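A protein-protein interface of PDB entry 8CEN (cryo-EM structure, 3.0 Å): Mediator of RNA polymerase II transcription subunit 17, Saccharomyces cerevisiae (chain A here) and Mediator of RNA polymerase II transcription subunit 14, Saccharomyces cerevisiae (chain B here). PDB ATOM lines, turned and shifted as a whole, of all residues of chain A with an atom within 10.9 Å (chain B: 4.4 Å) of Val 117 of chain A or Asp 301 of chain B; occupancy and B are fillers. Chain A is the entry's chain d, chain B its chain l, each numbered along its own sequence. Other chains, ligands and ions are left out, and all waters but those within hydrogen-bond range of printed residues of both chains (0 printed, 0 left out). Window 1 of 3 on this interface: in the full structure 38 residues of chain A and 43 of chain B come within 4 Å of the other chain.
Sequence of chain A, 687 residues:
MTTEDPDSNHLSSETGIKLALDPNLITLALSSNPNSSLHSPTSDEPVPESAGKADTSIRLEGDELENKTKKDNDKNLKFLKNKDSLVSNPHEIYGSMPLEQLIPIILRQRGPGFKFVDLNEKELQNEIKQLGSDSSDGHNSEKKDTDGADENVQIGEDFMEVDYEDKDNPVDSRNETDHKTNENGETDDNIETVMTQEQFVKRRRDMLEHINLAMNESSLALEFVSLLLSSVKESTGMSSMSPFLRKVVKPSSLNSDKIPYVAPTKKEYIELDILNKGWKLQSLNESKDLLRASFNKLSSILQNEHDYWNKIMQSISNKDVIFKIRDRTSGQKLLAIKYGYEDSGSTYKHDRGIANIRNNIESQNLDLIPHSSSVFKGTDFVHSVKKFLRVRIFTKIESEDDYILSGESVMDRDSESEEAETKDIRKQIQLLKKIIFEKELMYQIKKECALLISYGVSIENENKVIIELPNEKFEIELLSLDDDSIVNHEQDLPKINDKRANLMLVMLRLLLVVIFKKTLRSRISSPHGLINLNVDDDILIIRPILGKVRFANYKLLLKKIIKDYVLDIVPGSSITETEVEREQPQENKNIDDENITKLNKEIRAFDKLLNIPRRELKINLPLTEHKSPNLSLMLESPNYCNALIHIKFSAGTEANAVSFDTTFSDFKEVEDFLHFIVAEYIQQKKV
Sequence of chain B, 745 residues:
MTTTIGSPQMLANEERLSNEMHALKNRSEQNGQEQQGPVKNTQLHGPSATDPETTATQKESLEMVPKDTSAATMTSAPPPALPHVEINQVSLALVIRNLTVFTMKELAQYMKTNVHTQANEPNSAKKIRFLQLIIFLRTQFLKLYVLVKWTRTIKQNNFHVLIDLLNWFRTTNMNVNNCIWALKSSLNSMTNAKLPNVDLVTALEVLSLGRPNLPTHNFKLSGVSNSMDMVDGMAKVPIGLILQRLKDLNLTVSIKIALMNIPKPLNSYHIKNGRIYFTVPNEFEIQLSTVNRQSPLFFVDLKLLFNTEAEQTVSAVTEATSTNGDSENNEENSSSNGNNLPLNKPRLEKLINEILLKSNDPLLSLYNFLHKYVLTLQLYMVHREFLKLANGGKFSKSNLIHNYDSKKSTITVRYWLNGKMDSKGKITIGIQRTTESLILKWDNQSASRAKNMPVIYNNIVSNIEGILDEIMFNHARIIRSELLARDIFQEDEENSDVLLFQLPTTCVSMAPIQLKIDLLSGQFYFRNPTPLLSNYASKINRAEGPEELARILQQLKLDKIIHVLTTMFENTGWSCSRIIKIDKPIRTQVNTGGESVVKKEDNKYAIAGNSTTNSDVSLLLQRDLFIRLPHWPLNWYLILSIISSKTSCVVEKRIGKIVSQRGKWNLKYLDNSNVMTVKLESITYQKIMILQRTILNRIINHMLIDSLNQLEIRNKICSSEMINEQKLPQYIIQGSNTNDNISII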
ATOM      1  N   ILE A 103      -3.979  25.206  10.521  1.00  0.00           N
ATOM      2  CA  ILE A 103      -4.349  25.244   9.095  1.00  0.00           C
ATOM      3  C   ILE A 103      -5.854  25.305   8.845  1.00  0.00           C
ATOM      4  O   ILE A 103      -6.273  26.076   7.965  1.00  0.00           O
ATOM      5  CB  ILE A 103      -3.653  24.104   8.337  1.00  0.00           C
ATOM      6  CG1 ILE A 103      -2.134  24.219   8.463  1.00  0.00           C
ATOM      7  CG2 ILE A 103      -4.033  24.097   6.861  1.00  0.00           C
ATOM      8  CD1 ILE A 103      -1.576  25.497   7.884  1.00  0.00           C
ATOM      9  N   ILE A 106      -6.850  28.806   9.363  1.00  0.00           N
ATOM     10  CA  ILE A 106      -6.327  29.603   8.254  1.00  0.00           C
ATOM     11  C   ILE A 106      -7.256  29.523   7.050  1.00  0.00           C
ATOM     12  O   ILE A 106      -7.610  30.545   6.449  1.00  0.00           O
ATOM     13  CB  ILE A 106      -4.901  29.144   7.895  1.00  0.00           C
ATOM     14  CG1 ILE A 106      -3.923  29.505   9.015  1.00  0.00           C
ATOM     15  CG2 ILE A 106      -4.466  29.696   6.541  1.00  0.00           C
ATOM     16  CD1 ILE A 106      -2.520  29.000   8.785  1.00  0.00           C
ATOM     17  N   LEU A 107      -7.677  28.306   6.693  1.00  0.00           N
ATOM     18  CA  LEU A 107      -8.537  28.125   5.526  1.00  0.00           C
ATOM     19  C   LEU A 107      -9.902  28.774   5.733  1.00  0.00           C
ATOM     20  O   LEU A 107     -10.427  29.446   4.833  1.00  0.00           O
ATOM     21  CB  LEU A 107      -8.688  26.635   5.217  1.00  0.00           C
ATOM     22  CG  LEU A 107      -7.401  25.935   4.775  1.00  0.00           C
ATOM     23  CD1 LEU A 107      -7.615  24.436   4.622  1.00  0.00           C
ATOM     24  CD2 LEU A 107      -6.868  26.546   3.494  1.00  0.00           C
ATOM     25  N   ARG A 110      -9.525  32.521   5.559  1.00  0.00           N
ATOM     26  CA  ARG A 110      -9.264  32.975   4.199  1.00  0.00           C
ATOM     27  C   ARG A 110     -10.516  32.915   3.334  1.00  0.00           C
ATOM     28  O   ARG A 110     -10.701  33.768   2.458  1.00  0.00           O
ATOM     29  CB  ARG A 110      -8.141  32.151   3.569  1.00  0.00           C
ATOM     30  CG  ARG A 110      -6.745  32.557   4.017  1.00  0.00           C
ATOM     31  CD  ARG A 110      -6.465  34.023   3.728  1.00  0.00           C
ATOM     32  NE  ARG A 110      -6.449  34.307   2.298  1.00  0.00           N
ATOM     33  CZ  ARG A 110      -6.295  35.516   1.776  1.00  0.00           C
ATOM     34  NH1 ARG A 110      -6.142  36.585   2.542  1.00  0.00           N
ATOM     35  NH2 ARG A 110      -6.294  35.657   0.454  1.00  0.00           N
ATOM     36  N   GLY A 113     -15.353  27.464   2.180  1.00  0.00           N
ATOM     37  CA  GLY A 113     -15.015  26.497   1.155  1.00  0.00           C
ATOM     38  C   GLY A 113     -13.641  26.685   0.557  1.00  0.00           C
ATOM     39  O   GLY A 113     -13.395  26.238  -0.566  1.00  0.00           O
ATOM     40  N   PHE A 114     -12.734  27.340   1.279  1.00  0.00           N
ATOM     41  CA  PHE A 114     -11.404  27.646   0.774  1.00  0.00           C
ATOM     42  C   PHE A 114     -10.490  26.448   0.995  1.00  0.00           C
ATOM     43  O   PHE A 114     -10.460  25.874   2.089  1.00  0.00           O
ATOM     44  CB  PHE A 114     -10.841  28.886   1.470  1.00  0.00           C
ATOM     45  CG  PHE A 114      -9.553  29.385   0.882  1.00  0.00           C
ATOM     46  CD1 PHE A 114      -9.552  30.122  -0.292  1.00  0.00           C
ATOM     47  CD2 PHE A 114      -8.345  29.130   1.507  1.00  0.00           C
ATOM     48  CE1 PHE A 114      -8.370  30.588  -0.834  1.00  0.00           C
ATOM     49  CE2 PHE A 114      -7.157  29.592   0.970  1.00  0.00           C
ATOM     50  CZ  PHE A 114      -7.170  30.322  -0.202  1.00  0.00           C
ATOM     51  N   LYS A 115      -9.754  26.073  -0.044  1.00  0.00           N
ATOM     52  CA  LYS A 115      -8.891  24.904  -0.018  1.00  0.00           C
ATOM     53  C   LYS A 115      -7.439  25.331   0.174  1.00  0.00           C
ATOM     54  O   LYS A 115      -7.074  26.491  -0.036  1.00  0.00           O
ATOM     55  CB  LYS A 115      -9.059  24.097  -1.315  1.00  0.00           C
ATOM     56  CG  LYS A 115      -8.629  22.629  -1.252  1.00  0.00           C
ATOM     57  CD  LYS A 115      -9.200  21.918  -0.030  1.00  0.00           C
ATOM     58  CE  LYS A 115     -10.695  21.666  -0.170  1.00  0.00           C
ATOM     59  NZ  LYS A 115     -11.257  20.991   1.033  1.00  0.00           N
ATOM     60  N   PHE A 116      -6.610  24.368   0.595  1.00  0.00           N
ATOM     61  CA  PHE A 116      -5.182  24.613   0.789  1.00  0.00           C
ATOM     62  C   PHE A 116      -4.491  24.958  -0.527  1.00  0.00           C
ATOM     63  O   PHE A 116      -3.472  25.659  -0.526  1.00  0.00           O
ATOM     64  CB  PHE A 116      -4.558  23.378   1.457  1.00  0.00           C
ATOM     65  CG  PHE A 116      -3.141  23.570   1.952  1.00  0.00           C
ATOM     66  CD1 PHE A 116      -2.050  23.451   1.098  1.00  0.00           C
ATOM     67  CD2 PHE A 116      -2.905  23.870   3.285  1.00  0.00           C
ATOM     68  CE1 PHE A 116      -0.762  23.630   1.565  1.00  0.00           C
ATOM     69  CE2 PHE A 116      -1.618  24.048   3.756  1.00  0.00           C
ATOM     70  CZ  PHE A 116      -0.547  23.928   2.893  1.00  0.00           C
ATOM     71  N   VAL A 117      -5.048  24.504  -1.651  1.00  0.00           N
ATOM     72  CA  VAL A 117      -4.404  24.661  -2.952  1.00  0.00           C
ATOM     73  C   VAL A 117      -4.349  26.129  -3.366  1.00  0.00           C
ATOM     74  O   VAL A 117      -3.358  26.588  -3.946  1.00  0.00           O
ATOM     75  CB  VAL A 117      -5.144  23.806  -3.998  1.00  0.00           C
ATOM     76  CG1 VAL A 117      -4.460  23.885  -5.357  1.00  0.00           C
ATOM     77  CG2 VAL A 117      -5.264  22.368  -3.516  1.00  0.00           C
ATOM     78  N   ASP A 118      -5.390  26.896  -3.047  1.00  0.00           N
ATOM     79  CA  ASP A 118      -5.564  28.239  -3.592  1.00  0.00           C
ATOM     80  C   ASP A 118      -4.709  29.301  -2.902  1.00  0.00           C
ATOM     81  O   ASP A 118      -4.879  30.489  -3.200  1.00  0.00           O
ATOM     82  CB  ASP A 118      -7.040  28.639  -3.526  1.00  0.00           C
ATOM     83  CG  ASP A 118      -7.948  27.633  -4.208  1.00  0.00           C
ATOM     84  OD1 ASP A 118      -7.547  27.082  -5.254  1.00  0.00           O
ATOM     85  OD2 ASP A 118      -9.062  27.395  -3.696  1.00  0.00           O
ATOM     86  N   LEU A 119      -3.814  28.923  -1.995  1.00  0.00           N
ATOM     87  CA  LEU A 119      -2.880  29.885  -1.429  1.00  0.00           C
ATOM     88  C   LEU A 119      -1.819  30.265  -2.460  1.00  0.00           C
ATOM     89  O   LEU A 119      -1.569  29.542  -3.427  1.00  0.00           O
ATOM     90  CB  LEU A 119      -2.221  29.319  -0.170  1.00  0.00           C
ATOM     91  CG  LEU A 119      -3.135  29.131   1.042  1.00  0.00           C
ATOM     92  CD1 LEU A 119      -2.419  28.369   2.146  1.00  0.00           C
ATOM     93  CD2 LEU A 119      -3.627  30.477   1.554  1.00  0.00           C
ATOM     94  N   ASN A 120      -1.201  31.430  -2.249  1.00  0.00           N
ATOM     95  CA  ASN A 120      -0.157  31.923  -3.141  1.00  0.00           C
ATOM     96  C   ASN A 120       0.629  33.012  -2.426  1.00  0.00           C
ATOM     97  O   ASN A 120       0.037  33.958  -1.893  1.00  0.00           O
ATOM     98  CB  ASN A 120      -0.755  32.467  -4.448  1.00  0.00           C
ATOM     99  CG  ASN A 120       0.261  32.540  -5.579  1.00  0.00           C
ATOM    100  OD1 ASN A 120       1.445  32.801  -5.360  1.00  0.00           O
ATOM    101  ND2 ASN A 120      -0.205  32.308  -6.801  1.00  0.00           N
ATOM    102  N   GLU A 121       1.961  32.884  -2.434  1.00  0.00           N
ATOM    103  CA  GLU A 121       2.805  33.907  -1.822  1.00  0.00           C
ATOM    104  C   GLU A 121       2.716  35.227  -2.575  1.00  0.00           C
ATOM    105  O   GLU A 121       2.782  36.294  -1.961  1.00  0.00           O
ATOM    106  CB  GLU A 121       4.259  33.441  -1.749  1.00  0.00           C
ATOM    107  CG  GLU A 121       4.542  32.444  -0.645  1.00  0.00           C
ATOM    108  CD  GLU A 121       4.460  31.017  -1.123  1.00  0.00           C
ATOM    109  OE1 GLU A 121       4.280  30.814  -2.342  1.00  0.00           O
ATOM    110  OE2 GLU A 121       4.585  30.103  -0.283  1.00  0.00           O
ATOM    111  N   LYS A 122       2.570  35.176  -3.902  1.00  0.00           N
ATOM    112  CA  LYS A 122       2.374  36.402  -4.672  1.00  0.00           C
ATOM    113  C   LYS A 122       1.054  37.076  -4.314  1.00  0.00           C
ATOM    114  O   LYS A 122       0.987  38.308  -4.207  1.00  0.00           O
ATOM    115  CB  LYS A 122       2.434  36.096  -6.168  1.00  0.00           C
ATOM    116  CG  LYS A 122       2.570  37.326  -7.050  1.00  0.00           C
ATOM    117  CD  LYS A 122       3.850  38.087  -6.746  1.00  0.00           C
ATOM    118  CE  LYS A 122       3.994  39.302  -7.646  1.00  0.00           C
ATOM    119  NZ  LYS A 122       2.964  40.339  -7.352  1.00  0.00           N
ATOM    120  N   GLU A 123      -0.003  36.277  -4.124  1.00  0.00           N
ATOM    121  CA  GLU A 123      -1.297  36.823  -3.727  1.00  0.00           C
ATOM    122  C   GLU A 123      -1.220  37.460  -2.345  1.00  0.00           C
ATOM    123  O   GLU A 123      -1.761  38.550  -2.123  1.00  0.00           O
ATOM    124  CB  GLU A 123      -2.360  35.724  -3.766  1.00  0.00           C
ATOM    125  CG  GLU A 123      -3.801  36.218  -3.775  1.00  0.00           C
ATOM    126  CD  GLU A 123      -4.357  36.466  -2.387  1.00  0.00           C
ATOM    127  OE1 GLU A 123      -3.896  35.806  -1.432  1.00  0.00           O
ATOM    128  OE2 GLU A 123      -5.260  37.318  -2.255  1.00  0.00           O
ATOM    129  N   LEU A 124      -0.525  36.811  -1.407  1.00  0.00           N
ATOM    130  CA  LEU A 124      -0.341  37.417  -0.091  1.00  0.00           C
ATOM    131  C   LEU A 124       0.519  38.675  -0.170  1.00  0.00           C
ATOM    132  O   LEU A 124       0.251  39.658   0.531  1.00  0.00           O
ATOM    133  CB  LEU A 124       0.272  36.407   0.874  1.00  0.00           C
ATOM    134  CG  LEU A 124      -0.546  35.140   1.117  1.00  0.00           C
ATOM    135  CD1 LEU A 124       0.233  34.189   1.995  1.00  0.00           C
ATOM    136  CD2 LEU A 124      -1.893  35.472   1.741  1.00  0.00           C
ATOM    137  N   ASN B 273       4.826  27.591  -2.482  1.00  0.00           N
ATOM    138  CA  ASN B 273       3.398  27.677  -2.154  1.00  0.00           C
ATOM    139  C   ASN B 273       2.974  26.574  -1.175  1.00  0.00           C
ATOM    140  O   ASN B 273       2.062  25.784  -1.429  1.00  0.00           O
ATOM    141  CB  ASN B 273       2.559  27.667  -3.446  1.00  0.00           C
ATOM    142  CG  ASN B 273       1.078  27.976  -3.218  1.00  0.00           C
ATOM    143  OD1 ASN B 273       0.625  28.182  -2.091  1.00  0.00           O
ATOM    144  ND2 ASN B 273       0.319  28.019  -4.308  1.00  0.00           N
ATOM    145  N   ARG B 275       3.965  23.768  -0.218  1.00  0.00           N
ATOM    146  CA  ARG B 275       3.914  22.369  -0.617  1.00  0.00           C
ATOM    147  C   ARG B 275       5.030  22.105  -1.622  1.00  0.00           C
ATOM    148  O   ARG B 275       5.815  22.995  -1.959  1.00  0.00           O
ATOM    149  CB  ARG B 275       2.538  22.026  -1.195  1.00  0.00           C
ATOM    150  CG  ARG B 275       2.235  22.659  -2.527  1.00  0.00           C
ATOM    151  CD  ARG B 275       0.766  22.505  -2.880  1.00  0.00           C
ATOM    152  NE  ARG B 275      -0.055  23.570  -2.320  1.00  0.00           N
ATOM    153  CZ  ARG B 275      -0.391  24.674  -2.973  1.00  0.00           C
ATOM    154  NH1 ARG B 275       0.001  24.887  -4.218  1.00  0.00           N
ATOM    155  NH2 ARG B 275      -1.138  25.588  -2.361  1.00  0.00           N
ATOM    156  N   ILE B 286       1.890  16.041  -9.021  1.00  0.00           N
ATOM    157  CA  ILE B 286       1.202  15.782  -7.760  1.00  0.00           C
ATOM    158  C   ILE B 286       1.841  16.639  -6.671  1.00  0.00           C
ATOM    159  O   ILE B 286       3.070  16.726  -6.573  1.00  0.00           O
ATOM    160  CB  ILE B 286       1.223  14.281  -7.409  1.00  0.00           C
ATOM    161  CG1 ILE B 286       0.557  14.020  -6.056  1.00  0.00           C
ATOM    162  CG2 ILE B 286       2.638  13.699  -7.484  1.00  0.00           C
ATOM    163  CD1 ILE B 286       0.327  12.555  -5.760  1.00  0.00           C
ATOM    164  N   GLN B 287       1.005  17.301  -5.874  1.00  0.00           N
ATOM    165  CA  GLN B 287       1.450  18.271  -4.885  1.00  0.00           C
ATOM    166  C   GLN B 287       1.130  17.763  -3.486  1.00  0.00           C
ATOM    167  O   GLN B 287      -0.006  17.341  -3.215  1.00  0.00           O
ATOM    168  CB  GLN B 287       0.795  19.630  -5.138  1.00  0.00           C
ATOM    169  CG  GLN B 287       0.616  19.932  -6.617  1.00  0.00           C
ATOM    170  CD  GLN B 287       0.031  21.305  -6.880  1.00  0.00           C
ATOM    171  OE1 GLN B 287      -0.401  21.997  -5.958  1.00  0.00           O
ATOM    172  NE2 GLN B 287       0.016  21.708  -8.144  1.00  0.00           N
ATOM    173  N   PHE B 299      -1.215  14.084   0.964  1.00  0.00           N
ATOM    174  CA  PHE B 299      -1.667  14.469  -0.365  1.00  0.00           C
ATOM    175  C   PHE B 299      -2.325  15.844  -0.328  1.00  0.00           C
ATOM    176  O   PHE B 299      -3.007  16.194   0.639  1.00  0.00           O
ATOM    177  CB  PHE B 299      -2.635  13.398  -0.871  1.00  0.00           C
ATOM    178  CG  PHE B 299      -3.452  13.800  -2.058  1.00  0.00           C
ATOM    179  CD1 PHE B 299      -2.914  13.760  -3.329  1.00  0.00           C
ATOM    180  CD2 PHE B 299      -4.779  14.167  -1.906  1.00  0.00           C
ATOM    181  CE1 PHE B 299      -3.675  14.108  -4.419  1.00  0.00           C
ATOM    182  CE2 PHE B 299      -5.545  14.518  -2.994  1.00  0.00           C
ATOM    183  CZ  PHE B 299      -4.994  14.484  -4.252  1.00  0.00           C
ATOM    184  N   VAL B 300      -2.127  16.629  -1.390  1.00  0.00           N
ATOM    185  CA  VAL B 300      -2.738  17.947  -1.496  1.00  0.00           C
ATOM    186  C   VAL B 300      -3.592  17.960  -2.753  1.00  0.00           C
ATOM    187  O   VAL B 300      -4.818  18.101  -2.669  1.00  0.00           O
ATOM    188  CB  VAL B 300      -1.680  19.065  -1.519  1.00  0.00           C
ATOM    189  CG1 VAL B 300      -2.312  20.395  -1.910  1.00  0.00           C
ATOM    190  CG2 VAL B 300      -1.002  19.177  -0.168  1.00  0.00           C
ATOM    191  N   ASP B 301      -2.965  17.787  -3.920  1.00  0.00           N
ATOM    192  CA  ASP B 301      -3.752  17.631  -5.145  1.00  0.00           C
ATOM    193  C   ASP B 301      -2.908  16.905  -6.186  1.00  0.00           C
ATOM    194  O   ASP B 301      -1.750  16.556  -5.944  1.00  0.00           O
ATOM    195  CB  ASP B 301      -4.289  18.976  -5.666  1.00  0.00           C
ATOM    196  CG  ASP B 301      -3.200  19.936  -6.094  1.00  0.00           C
ATOM    197  OD1 ASP B 301      -2.563  19.703  -7.142  1.00  0.00           O
ATOM    198  OD2 ASP B 301      -2.974  20.927  -5.372  1.00  0.00           O
ATOM    199  N   LEU B 302      -3.509  16.663  -7.350  1.00  0.00           N
ATOM    200  CA  LEU B 302      -2.796  16.085  -8.480  1.00  0.00           C
ATOM    201  C   LEU B 302      -3.441  16.546  -9.779  1.00  0.00           C
ATOM    202  O   LEU B 302      -4.669  16.604  -9.889  1.00  0.00           O
ATOM    203  CB  LEU B 302      -2.744  14.549  -8.390  1.00  0.00           C
ATOM    204  CG  LEU B 302      -3.995  13.664  -8.355  1.00  0.00           C
ATOM    205  CD1 LEU B 302      -4.440  13.236  -9.733  1.00  0.00           C
ATOM    206  CD2 LEU B 302      -3.707  12.429  -7.522  1.00  0.00           C
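NH2 of Arg 275 of chain B is in hydrogen-bond range of O of Phe 116 of chain A (3.0 Å). The backbone carbonyl oxygen (O) of Val 117 of chain A sits at hydrogen-bond distance from the guanidinium group (NH2) of Arg 275 of chain B (2.9 Å). O of Leu 119 of chain A is in hydrogen-bond range of ND2 of Asn 273 of chain B, 2.6 Å away. N of Asn 273 of chain B sits close to OE1 of Glu 121 of chain A (3.3 Å).
The backbone NH (N) of Lys 122 of chain A is in hydrogen-bond range of the side-chain amide oxygen (OD1) of Asn 120 of chain A (3.0 Å). NH2 of Arg 275 of chain B is in hydrogen-bond range of OD1 of Asn 273 of chain B (3.1 Å). The guanidinium group (NH1) of Arg 275 of chain B lies close to the side-chain amide oxygen (OE1) of Gln 287 of chain B (3.4 Å). The backbone NH (N) of Val 300 of chain B sits at hydrogen-bond distance from the backbone carbonyl oxygen (O) of Gln 287 of chain B. OD2 of Asp 301 of chain B sits close to OE1 of Gln 287 of chain B (2.8 Å).
Among the printed residues, pairs that only touch across the chains: Val 117 of chain A with Asn 273 of chain B, Val 117 of chain A with Val 300 of chain B, Val 117 of chain A with Asp 301 of chain B and Asn 120 of chain A with Asn 273 of chain B.
Of chain B, only Asn 273 (3.96 Å), Arg 275 (2.9 Å), Val 300 (3.9 Å) and Asp 301 (3.3 Å) come within 4 Å of Val 117 of chain A. No residue of chain A comes within 4 Å of Ile 286 of chain B. No residue of chain A comes within 4 Å of Gln 287 of chain B. Of chain A, only Val 117 (3.9 Å) comes within 4 Å of Val 300 of chain B. No residue of chain A comes within 4 Å of Leu 302 of chain B. Of the printed residues of chain A, Asn 273 of chain B touches Val 117, Leu 119, Asn 120 and Glu 121. Printed residues of chain B within 4 Å of Leu 119 of chain A: Asn 273. Of the printed residues of chain B, Glu 121 of chain A touches Asn 273. Gly 113 of chain A touches none of the printed residues of chain B. Lys 122 of chain A touches none of the printed residues of chain B. The nearest printed residue of chain B that does not touch Val 117 of chain A is Gln 287 of chain B (4.5 Å). The nearest printed residue of chain B that does not touch Asn 120 of chain A is Arg 275 of chain B (5.8 Å).
Of the 16 printed residues of chain A, 5 touch a printed residue of chain B. Hydrophobic or aromatic side chains of chain B that line the printed part of chain A: Val 300.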
